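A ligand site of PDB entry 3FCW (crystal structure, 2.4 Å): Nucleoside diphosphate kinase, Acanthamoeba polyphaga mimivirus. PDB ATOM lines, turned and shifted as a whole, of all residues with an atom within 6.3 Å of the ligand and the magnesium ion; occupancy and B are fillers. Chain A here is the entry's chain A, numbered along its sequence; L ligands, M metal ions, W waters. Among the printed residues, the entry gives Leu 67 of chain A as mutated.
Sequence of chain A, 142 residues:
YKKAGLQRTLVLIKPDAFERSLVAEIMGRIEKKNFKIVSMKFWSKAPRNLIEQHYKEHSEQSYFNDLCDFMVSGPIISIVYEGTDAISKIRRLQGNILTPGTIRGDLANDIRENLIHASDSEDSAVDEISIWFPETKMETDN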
ATOM      1  N   LYS A  14     -23.394 -17.603 -22.189  1.00  0.00           N
ATOM      2  CA  LYS A  14     -24.111 -18.323 -21.150  1.00  0.00           C
ATOM      3  C   LYS A  14     -24.312 -17.459 -19.891  1.00  0.00           C
ATOM      4  O   LYS A  14     -23.660 -16.430 -19.732  1.00  0.00           O
ATOM      5  CB  LYS A  14     -23.391 -19.633 -20.833  1.00  0.00           C
ATOM      6  CG  LYS A  14     -23.123 -20.471 -22.086  1.00  0.00           C
ATOM      7  CD  LYS A  14     -22.514 -21.807 -21.730  1.00  0.00           C
ATOM      8  CE  LYS A  14     -22.555 -22.747 -22.916  1.00  0.00           C
ATOM      9  NZ  LYS A  14     -22.039 -24.100 -22.527  1.00  0.00           N
ATOM     10  N   TYR A  55     -30.031 -28.123 -27.126  1.00  0.00           N
ATOM     11  CA  TYR A  55     -29.252 -29.212 -26.554  1.00  0.00           C
ATOM     12  C   TYR A  55     -29.905 -30.598 -26.746  1.00  0.00           C
ATOM     13  O   TYR A  55     -29.651 -31.516 -25.963  1.00  0.00           O
ATOM     14  CB  TYR A  55     -28.966 -28.943 -25.083  1.00  0.00           C
ATOM     15  CG  TYR A  55     -27.822 -27.981 -24.843  1.00  0.00           C
ATOM     16  CD1 TYR A  55     -28.004 -26.831 -24.091  1.00  0.00           C
ATOM     17  CD2 TYR A  55     -26.564 -28.231 -25.371  1.00  0.00           C
ATOM     18  CE1 TYR A  55     -26.949 -25.954 -23.856  1.00  0.00           C
ATOM     19  CE2 TYR A  55     -25.504 -27.362 -25.150  1.00  0.00           C
ATOM     20  CZ  TYR A  55     -25.705 -26.222 -24.393  1.00  0.00           C
ATOM     21  OH  TYR A  55     -24.657 -25.360 -24.173  1.00  0.00           O
ATOM     22  N   HIS A  58     -28.068 -33.842 -26.613  1.00  0.00           N
ATOM     23  CA  HIS A  58     -27.591 -34.236 -25.287  1.00  0.00           C
ATOM     24  C   HIS A  58     -28.724 -34.734 -24.394  1.00  0.00           C
ATOM     25  O   HIS A  58     -28.531 -34.899 -23.194  1.00  0.00           O
ATOM     26  CB  HIS A  58     -26.897 -33.058 -24.572  1.00  0.00           C
ATOM     27  CG  HIS A  58     -25.784 -32.431 -25.348  1.00  0.00           C
ATOM     28  ND1 HIS A  58     -24.445 -32.607 -25.020  1.00  0.00           N
ATOM     29  CD2 HIS A  58     -25.776 -31.602 -26.422  1.00  0.00           C
ATOM     30  CE1 HIS A  58     -23.689 -31.940 -25.858  1.00  0.00           C
ATOM     31  NE2 HIS A  58     -24.485 -31.314 -26.731  1.00  0.00           N
ATOM     32  N   SER A  62     -26.386 -37.659 -18.383  1.00  0.00           N
ATOM     33  CA  SER A  62     -26.501 -37.362 -16.963  1.00  0.00           C
ATOM     34  C   SER A  62     -26.693 -35.873 -16.719  1.00  0.00           C
ATOM     35  O   SER A  62     -27.606 -35.462 -15.997  1.00  0.00           O
ATOM     36  CB  SER A  62     -25.251 -37.854 -16.234  1.00  0.00           C
ATOM     37  OG  SER A  62     -24.100 -37.585 -17.019  1.00  0.00           O
ATOM     38  N   TYR A  63     -25.840 -35.057 -17.351  1.00  0.00           N
ATOM     39  CA  TYR A  63     -25.812 -33.617 -17.089  1.00  0.00           C
ATOM     40  C   TYR A  63     -26.951 -32.856 -17.748  1.00  0.00           C
ATOM     41  O   TYR A  63     -27.063 -31.644 -17.563  1.00  0.00           O
ATOM     42  CB  TYR A  63     -24.463 -33.013 -17.531  1.00  0.00           C
ATOM     43  CG  TYR A  63     -24.172 -33.191 -19.008  1.00  0.00           C
ATOM     44  CD1 TYR A  63     -24.748 -32.363 -19.953  1.00  0.00           C
ATOM     45  CD2 TYR A  63     -23.322 -34.203 -19.437  1.00  0.00           C
ATOM     46  CE1 TYR A  63     -24.474 -32.536 -21.304  1.00  0.00           C
ATOM     47  CE2 TYR A  63     -23.055 -34.380 -20.781  1.00  0.00           C
ATOM     48  CZ  TYR A  63     -23.627 -33.549 -21.704  1.00  0.00           C
ATOM     49  OH  TYR A  63     -23.356 -33.735 -23.035  1.00  0.00           O
ATOM     50  N   ASP A  66     -29.283 -30.603 -15.374  1.00  0.00           N
ATOM     51  CA  ASP A  66     -28.477 -29.591 -14.696  1.00  0.00           C
ATOM     52  C   ASP A  66     -28.096 -28.484 -15.682  1.00  0.00           C
ATOM     53  O   ASP A  66     -28.109 -27.306 -15.347  1.00  0.00           O
ATOM     54  CB  ASP A  66     -27.218 -30.218 -14.099  1.00  0.00           C
ATOM     55  CG  ASP A  66     -27.549 -31.227 -13.019  1.00  0.00           C
ATOM     56  OD1 ASP A  66     -28.537 -30.994 -12.274  1.00  0.00           O
ATOM     57  OD2 ASP A  66     -26.826 -32.253 -12.912  1.00  0.00           O
ATOM     58  N   LEU A  67     -27.756 -28.892 -16.893  1.00  0.00           N
ATOM     59  CA  LEU A  67     -27.321 -27.962 -17.923  1.00  0.00           C
ATOM     60  C   LEU A  67     -28.468 -27.063 -18.337  1.00  0.00           C
ATOM     61  O   LEU A  67     -28.303 -25.853 -18.502  1.00  0.00           O
ATOM     62  CB  LEU A  67     -26.752 -28.723 -19.123  1.00  0.00           C
ATOM     63  CG  LEU A  67     -26.664 -27.945 -20.425  1.00  0.00           C
ATOM     64  CD1 LEU A  67     -25.711 -26.749 -20.303  1.00  0.00           C
ATOM     65  CD2 LEU A  67     -26.247 -28.858 -21.559  1.00  0.00           C
ATOM     66  N   PHE A  70     -29.176 -24.548 -15.423  1.00  0.00           N
ATOM     67  CA  PHE A  70     -28.186 -23.484 -15.543  1.00  0.00           C
ATOM     68  C   PHE A  70     -28.512 -22.534 -16.702  1.00  0.00           C
ATOM     69  O   PHE A  70     -28.528 -21.315 -16.536  1.00  0.00           O
ATOM     70  CB  PHE A  70     -26.788 -24.106 -15.694  1.00  0.00           C
ATOM     71  CG  PHE A  70     -25.744 -23.159 -16.218  1.00  0.00           C
ATOM     72  CD1 PHE A  70     -25.068 -23.447 -17.392  1.00  0.00           C
ATOM     73  CD2 PHE A  70     -25.413 -22.011 -15.531  1.00  0.00           C
ATOM     74  CE1 PHE A  70     -24.094 -22.584 -17.883  1.00  0.00           C
ATOM     75  CE2 PHE A  70     -24.441 -21.148 -16.007  1.00  0.00           C
ATOM     76  CZ  PHE A  70     -23.775 -21.431 -17.190  1.00  0.00           C
ATOM     77  N   MET A  71     -28.807 -23.111 -17.871  1.00  0.00           N
ATOM     78  CA  MET A  71     -29.087 -22.295 -19.058  1.00  0.00           C
ATOM     79  C   MET A  71     -30.285 -21.367 -18.879  1.00  0.00           C
ATOM     80  O   MET A  71     -30.425 -20.384 -19.614  1.00  0.00           O
ATOM     81  CB  MET A  71     -29.251 -23.179 -20.297  1.00  0.00           C
ATOM     82  CG  MET A  71     -27.937 -23.785 -20.795  1.00  0.00           C
ATOM     83  SD  MET A  71     -26.629 -22.560 -21.065  1.00  0.00           S
ATOM     84  CE  MET A  71     -27.181 -21.776 -22.577  1.00  0.00           C
ATOM     85  N   ARG A  91     -15.053 -21.686 -32.899  1.00  0.00           N
ATOM     86  CA  ARG A  91     -14.845 -22.845 -32.036  1.00  0.00           C
ATOM     87  C   ARG A  91     -13.463 -22.887 -31.380  1.00  0.00           C
ATOM     88  O   ARG A  91     -13.338 -23.218 -30.207  1.00  0.00           O
ATOM     89  CB  ARG A  91     -15.104 -24.138 -32.792  1.00  0.00           C
ATOM     90  CG  ARG A  91     -16.392 -24.823 -32.410  1.00  0.00           C
ATOM     91  CD  ARG A  91     -16.157 -25.931 -31.394  1.00  0.00           C
ATOM     92  NE  ARG A  91     -17.290 -26.084 -30.476  1.00  0.00           N
ATOM     93  CZ  ARG A  91     -17.460 -27.100 -29.636  1.00  0.00           C
ATOM     94  NH1 ARG A  91     -16.594 -28.105 -29.601  1.00  0.00           N
ATOM     95  NH2 ARG A  91     -18.515 -27.121 -28.842  1.00  0.00           N
ATOM     96  N   GLN A  94     -13.276 -20.337 -28.714  1.00  0.00           N
ATOM     97  CA  GLN A  94     -13.939 -20.807 -27.506  1.00  0.00           C
ATOM     98  C   GLN A  94     -13.039 -21.733 -26.726  1.00  0.00           C
ATOM     99  O   GLN A  94     -12.915 -21.604 -25.509  1.00  0.00           O
ATOM    100  CB  GLN A  94     -15.255 -21.522 -27.818  1.00  0.00           C
ATOM    101  CG  GLN A  94     -15.544 -22.682 -26.874  1.00  0.00           C
ATOM    102  CD  GLN A  94     -16.822 -23.423 -27.240  1.00  0.00           C
ATOM    103  OE1 GLN A  94     -17.915 -22.885 -27.141  1.00  0.00           O
ATOM    104  NE2 GLN A  94     -16.674 -24.678 -27.678  1.00  0.00           N
ATOM    105  N   GLY A  95     -12.395 -22.671 -27.427  1.00  0.00           N
ATOM    106  CA  GLY A  95     -11.416 -23.556 -26.823  1.00  0.00           C
ATOM    107  C   GLY A  95     -11.972 -24.356 -25.658  1.00  0.00           C
ATOM    108  O   GLY A  95     -13.132 -24.750 -25.681  1.00  0.00           O
ATOM    109  N   ARG A 104     -12.547 -20.031 -22.929  1.00  0.00           N
ATOM    110  CA  ARG A 104     -12.651 -20.947 -21.803  1.00  0.00           C
ATOM    111  C   ARG A 104     -11.310 -21.159 -21.099  1.00  0.00           C
ATOM    112  O   ARG A 104     -11.251 -21.296 -19.869  1.00  0.00           O
ATOM    113  CB  ARG A 104     -13.236 -22.288 -22.243  1.00  0.00           C
ATOM    114  CG  ARG A 104     -14.677 -22.195 -22.697  1.00  0.00           C
ATOM    115  CD  ARG A 104     -15.196 -23.545 -23.102  1.00  0.00           C
ATOM    116  NE  ARG A 104     -16.571 -23.483 -23.551  1.00  0.00           N
ATOM    117  CZ  ARG A 104     -17.259 -24.539 -23.984  1.00  0.00           C
ATOM    118  NH1 ARG A 104     -16.665 -25.730 -24.002  1.00  0.00           N
ATOM    119  NH2 ARG A 104     -18.504 -24.415 -24.383  1.00  0.00           N
ATOM    120  N   ILE A 111     -16.971 -27.749 -15.860  1.00  0.00           N
ATOM    121  CA  ILE A 111     -17.520 -28.557 -16.947  1.00  0.00           C
ATOM    122  C   ILE A 111     -18.867 -28.045 -17.421  1.00  0.00           C
ATOM    123  O   ILE A 111     -19.265 -28.313 -18.555  1.00  0.00           O
ATOM    124  CB  ILE A 111     -17.742 -30.034 -16.540  1.00  0.00           C
ATOM    125  CG1 ILE A 111     -18.141 -30.145 -15.061  1.00  0.00           C
ATOM    126  CG2 ILE A 111     -16.522 -30.884 -16.871  1.00  0.00           C
ATOM    127  CD1 ILE A 111     -18.595 -31.545 -14.637  1.00  0.00           C
ATOM    128  N   ARG A 112     -19.578 -27.324 -16.570  1.00  0.00           N
ATOM    129  CA  ARG A 112     -20.912 -26.860 -16.916  1.00  0.00           C
ATOM    130  C   ARG A 112     -20.951 -25.354 -17.177  1.00  0.00           C
ATOM    131  O   ARG A 112     -21.385 -24.918 -18.227  1.00  0.00           O
ATOM    132  CB  ARG A 112     -21.923 -27.240 -15.823  1.00  0.00           C
ATOM    133  CG  ARG A 112     -23.374 -27.118 -16.256  1.00  0.00           C
ATOM    134  CD  ARG A 112     -24.321 -27.391 -15.097  1.00  0.00           C
ATOM    135  NE  ARG A 112     -24.432 -26.212 -14.252  1.00  0.00           N
ATOM    136  CZ  ARG A 112     -24.556 -26.242 -12.936  1.00  0.00           C
ATOM    137  NH1 ARG A 112     -24.567 -27.426 -12.321  1.00  0.00           N
ATOM    138  NH2 ARG A 112     -24.660 -25.118 -12.241  1.00  0.00           N
ATOM    139  N   GLU A 113     -20.493 -24.564 -16.198  1.00  0.00           N
ATOM    140  CA  GLU A 113     -20.467 -23.111 -16.340  1.00  0.00           C
ATOM    141  C   GLU A 113     -19.214 -22.693 -17.103  1.00  0.00           C
ATOM    142  O   GLU A 113     -18.163 -22.451 -16.512  1.00  0.00           O
ATOM    143  CB  GLU A 113     -20.548 -22.441 -14.969  1.00  0.00           C
ATOM    144  CG  GLU A 113     -21.408 -23.219 -13.960  1.00  0.00           C
ATOM    145  CD  GLU A 113     -22.065 -22.327 -12.920  1.00  0.00           C
ATOM    146  OE1 GLU A 113     -21.854 -21.090 -12.974  1.00  0.00           O
ATOM    147  OE2 GLU A 113     -22.796 -22.854 -12.055  1.00  0.00           O
ATOM    148  N   ASN A 114     -19.333 -22.637 -18.413  1.00  0.00           N
ATOM    149  CA  ASN A 114     -18.175 -22.342 -19.253  1.00  0.00           C
ATOM    150  C   ASN A 114     -18.361 -21.172 -20.213  1.00  0.00           C
ATOM    151  O   ASN A 114     -17.751 -21.129 -21.284  1.00  0.00           O
ATOM    152  CB  ASN A 114     -17.646 -23.596 -19.961  1.00  0.00           C
ATOM    153  CG  ASN A 114     -18.706 -24.316 -20.774  1.00  0.00           C
ATOM    154  OD1 ASN A 114     -19.715 -23.741 -21.178  1.00  0.00           O
ATOM    155  ND2 ASN A 114     -18.481 -25.604 -21.022  1.00  0.00           N
ATOM    156  N   ILE A 116     -19.662 -19.852 -22.710  1.00  0.00           N
ATOM    157  CA  ILE A 116     -20.001 -19.703 -24.124  1.00  0.00           C
ATOM    158  C   ILE A 116     -20.290 -21.023 -24.833  1.00  0.00           C
ATOM    159  O   ILE A 116     -19.728 -22.065 -24.515  1.00  0.00           O
ATOM    160  CB  ILE A 116     -18.860 -19.015 -24.867  1.00  0.00           C
ATOM    161  CG1 ILE A 116     -19.193 -18.876 -26.358  1.00  0.00           C
ATOM    162  CG2 ILE A 116     -17.539 -19.764 -24.652  1.00  0.00           C
ATOM    163  CD1 ILE A 116     -18.135 -18.166 -27.130  1.00  0.00           C
ATOM    164  N   HIS A 117     -21.189 -20.948 -25.819  1.00  0.00           N
ATOM    165  CA  HIS A 117     -21.405 -22.014 -26.776  1.00  0.00           C
ATOM    166  C   HIS A 117     -21.152 -21.537 -28.201  1.00  0.00           C
ATOM    167  O   HIS A 117     -21.509 -20.415 -28.568  1.00  0.00           O
ATOM    168  CB  HIS A 117     -22.832 -22.566 -26.688  1.00  0.00           C
ATOM    169  CG  HIS A 117     -23.208 -23.417 -27.867  1.00  0.00           C
ATOM    170  ND1 HIS A 117     -23.222 -24.786 -27.821  1.00  0.00           N
ATOM    171  CD2 HIS A 117     -23.520 -23.067 -29.136  1.00  0.00           C
ATOM    172  CE1 HIS A 117     -23.567 -25.254 -29.013  1.00  0.00           C
ATOM    173  NE2 HIS A 117     -23.742 -24.235 -29.828  1.00  0.00           N
ATOM    174  N   ALA A 118     -20.538 -22.402 -29.002  1.00  0.00           N
ATOM    175  CA  ALA A 118     -20.353 -22.111 -30.418  1.00  0.00           C
ATOM    176  C   ALA A 118     -20.671 -23.357 -31.242  1.00  0.00           C
ATOM    177  O   ALA A 118     -20.303 -24.460 -30.851  1.00  0.00           O
ATOM    178  CB  ALA A 118     -18.930 -21.633 -30.679  1.00  0.00           C
ATOM    179  N   ASP A 120     -20.498 -26.345 -33.774  1.00  0.00           N
ATOM    180  CA  ASP A 120     -19.320 -27.127 -34.078  1.00  0.00           C
ATOM    181  C   ASP A 120     -19.277 -27.704 -35.486  1.00  0.00           C
ATOM    182  O   ASP A 120     -18.262 -28.258 -35.897  1.00  0.00           O
ATOM    183  CB  ASP A 120     -19.122 -28.243 -33.044  1.00  0.00           C
ATOM    184  CG  ASP A 120     -20.187 -29.294 -33.122  1.00  0.00           C
ATOM    185  OD1 ASP A 120     -21.115 -29.141 -33.951  1.00  0.00           O
ATOM    186  OD2 ASP A 120     -20.109 -30.288 -32.351  1.00  0.00           O
HETATM  187  N1  LIG L   1     -21.895 -29.870 -19.850  1.00  0.00           N
HETATM  188  C1  LIG L   1     -22.082 -30.187 -18.499  1.00  0.00           C
HETATM  189  N2  LIG L   1     -21.495 -31.291 -17.953  1.00  0.00           N
HETATM  190  C2  LIG L   1     -20.703 -32.102 -18.722  1.00  0.00           C
HETATM  191  C3  LIG L   1     -20.505 -31.791 -20.064  1.00  0.00           C
HETATM  192  C4  LIG L   1     -21.273 -30.777 -20.652  1.00  0.00           C
HETATM  193  O1  LIG L   1     -22.785 -29.499 -17.769  1.00  0.00           O
HETATM  194  O2  LIG L   1     -20.189 -33.087 -18.186  1.00  0.00           O
HETATM  195  C5  LIG L   1     -22.534 -28.681 -20.434  1.00  0.00           C
HETATM  196  C6  LIG L   1     -21.457 -27.643 -20.760  1.00  0.00           C
HETATM  197  O3  LIG L   1     -21.930 -26.333 -20.528  1.00  0.00           O
HETATM  198  C7  LIG L   1     -21.204 -27.853 -22.249  1.00  0.00           C
HETATM  199  C8  LIG L   1     -22.525 -28.415 -22.762  1.00  0.00           C
HETATM  200  O4  LIG L   1     -23.170 -29.014 -21.656  1.00  0.00           O
HETATM  201  O5  LIG L   1     -20.868 -26.661 -22.903  1.00  0.00           O
HETATM  202  C9  LIG L   1     -22.335 -29.397 -23.913  1.00  0.00           C
HETATM  203  O6  LIG L   1     -21.351 -30.377 -23.595  1.00  0.00           O
HETATM  204  P1  LIG L   1     -20.091 -30.509 -24.589  1.00  0.00           P
HETATM  205  O7  LIG L   1     -20.554 -30.692 -25.996  1.00  0.00           O
HETATM  206  O8  LIG L   1     -19.171 -31.567 -24.116  1.00  0.00           O
HETATM  207  O9  LIG L   1     -19.402 -29.069 -24.406  1.00  0.00           O
HETATM  208  P2  LIG L   1     -19.025 -28.083 -25.624  1.00  0.00           P
HETATM  209  O10 LIG L   1     -17.550 -28.019 -25.674  1.00  0.00           O
HETATM  210  O11 LIG L   1     -19.674 -26.768 -25.373  1.00  0.00           O
HETATM  211  O12 LIG L   1     -19.516 -28.589 -26.917  1.00  0.00           O
HETATM  212 MG    MG M   1     -19.851 -30.239 -28.544  1.00  0.00          MG
HETATM  213  O   HOH W   1     -21.969 -28.609 -27.797  1.00  0.00           O
HETATM  214  O   HOH W   2     -20.497 -33.812 -23.398  1.00  0.00           O
HETATM  215  O   HOH W   3     -22.299 -25.663 -25.317  1.00  0.00           O
HETATM  216  O   HOH W   4     -14.816 -28.218 -26.920  1.00  0.00           O
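Water W2 lies within hydrogen-bond range of O8 of the ligand and OH of Tyr 63.
Water W3 lies within hydrogen-bond range of the side-chain hydroxyl of Tyr 55 (2.6 Å), a ring nitrogen (ND1) of His 117 (2.8 Å), an oxygen (O11) of the ligand (2.8 Å) and the side-chain amino group of Lys 14 (3.2 Å).
Water W4 bridges an oxygen (O10) of the ligand and the guanidinium group of Arg 91.
An oxygen (O12) of the ligand is bound to the magnesium ion.
The magnesium ion has one donor atom within binding distance.
Slightly farther from the magnesium ion lies an oxygen (O7) of the ligand (2.7 Å).
Slightly farther from the magnesium ion lies water W1 (2.8 Å).
The side-chain hydroxyl of Tyr 55 lies within hydrogen-bond range of the side-chain amino group of Lys 14, 3.3 Å away.
OE1 of Gln 94 sits close to O of Ile 116, 3.3 Å away.
The side-chain amino group (NZ) of Lys 14 sits at hydrogen-bond distance from the side-chain amide oxygen (OD1) of Asn 114 (2.7 Å).
The side-chain amide oxygen (OE1) of Gln 94 lies within hydrogen-bond range of the backbone NH (N) of Ala 118, at 3.3 Å.
The backbone carbonyl oxygen (O) of Asn 114 is in hydrogen-bond range of the guanidinium group (NE) of Arg 104, at 3.5 Å.
The backbone carbonyl oxygen (O) of Gln 94 lies within hydrogen-bond range of the backbone NH (N) of Arg 104.
A ring nitrogen (ND1) of His 58 is in hydrogen-bond range of the side-chain hydroxyl (OH) of Tyr 63 (2.5 Å).
The guanidinium group (NE) of Arg 91 sits close to the side-chain amide nitrogen (NE2) of Gln 94.
NH2 of Arg 91 touches the magnesium ion, 3.4 Å away.
Asp 120 touches the magnesium ion.
Of the 21 residues printed, 2 come within 4 Å of the magnesium ion.
Along chain A the residues within 4 Å of the magnesium ion span positions 91 to 120.
The nearest printed residue that does not touch the magnesium ion is His 58 (5.0 Å).
O of Ile 111 lies close to N1 of the ligand (3.3 Å).
Residues that only touch the ligand: Tyr 55 (3.96 Å), His 58 (3.4 Å), Tyr 63 (3.4 Å), Leu 67 (3.1 Å) and Gln 94 (3.99 Å).
Hydrophobic or aromatic side chains within 4 Å of the ligand: Tyr 55, His 58, Tyr 63 and Leu 67.
O5 of the ligand is in hydrogen-bond range of NZ of Lys 14 (2.8 Å).
An oxygen (O11) of the ligand lies within salt-bridge range of the guanidinium group (NH2) of Arg 104 (2.8 Å).
The backbone carbonyl oxygen (O) of Arg 112 sits at hydrogen-bond distance from an oxygen (O3) of the ligand, 2.8 Å away.
The side-chain amide nitrogen (ND2) of Asn 114 lies within hydrogen-bond range of an oxygen (O5) of the ligand.
NH2 of Arg 91 lies within salt-bridge range of O10 of the ligand, at 3.4 Å.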
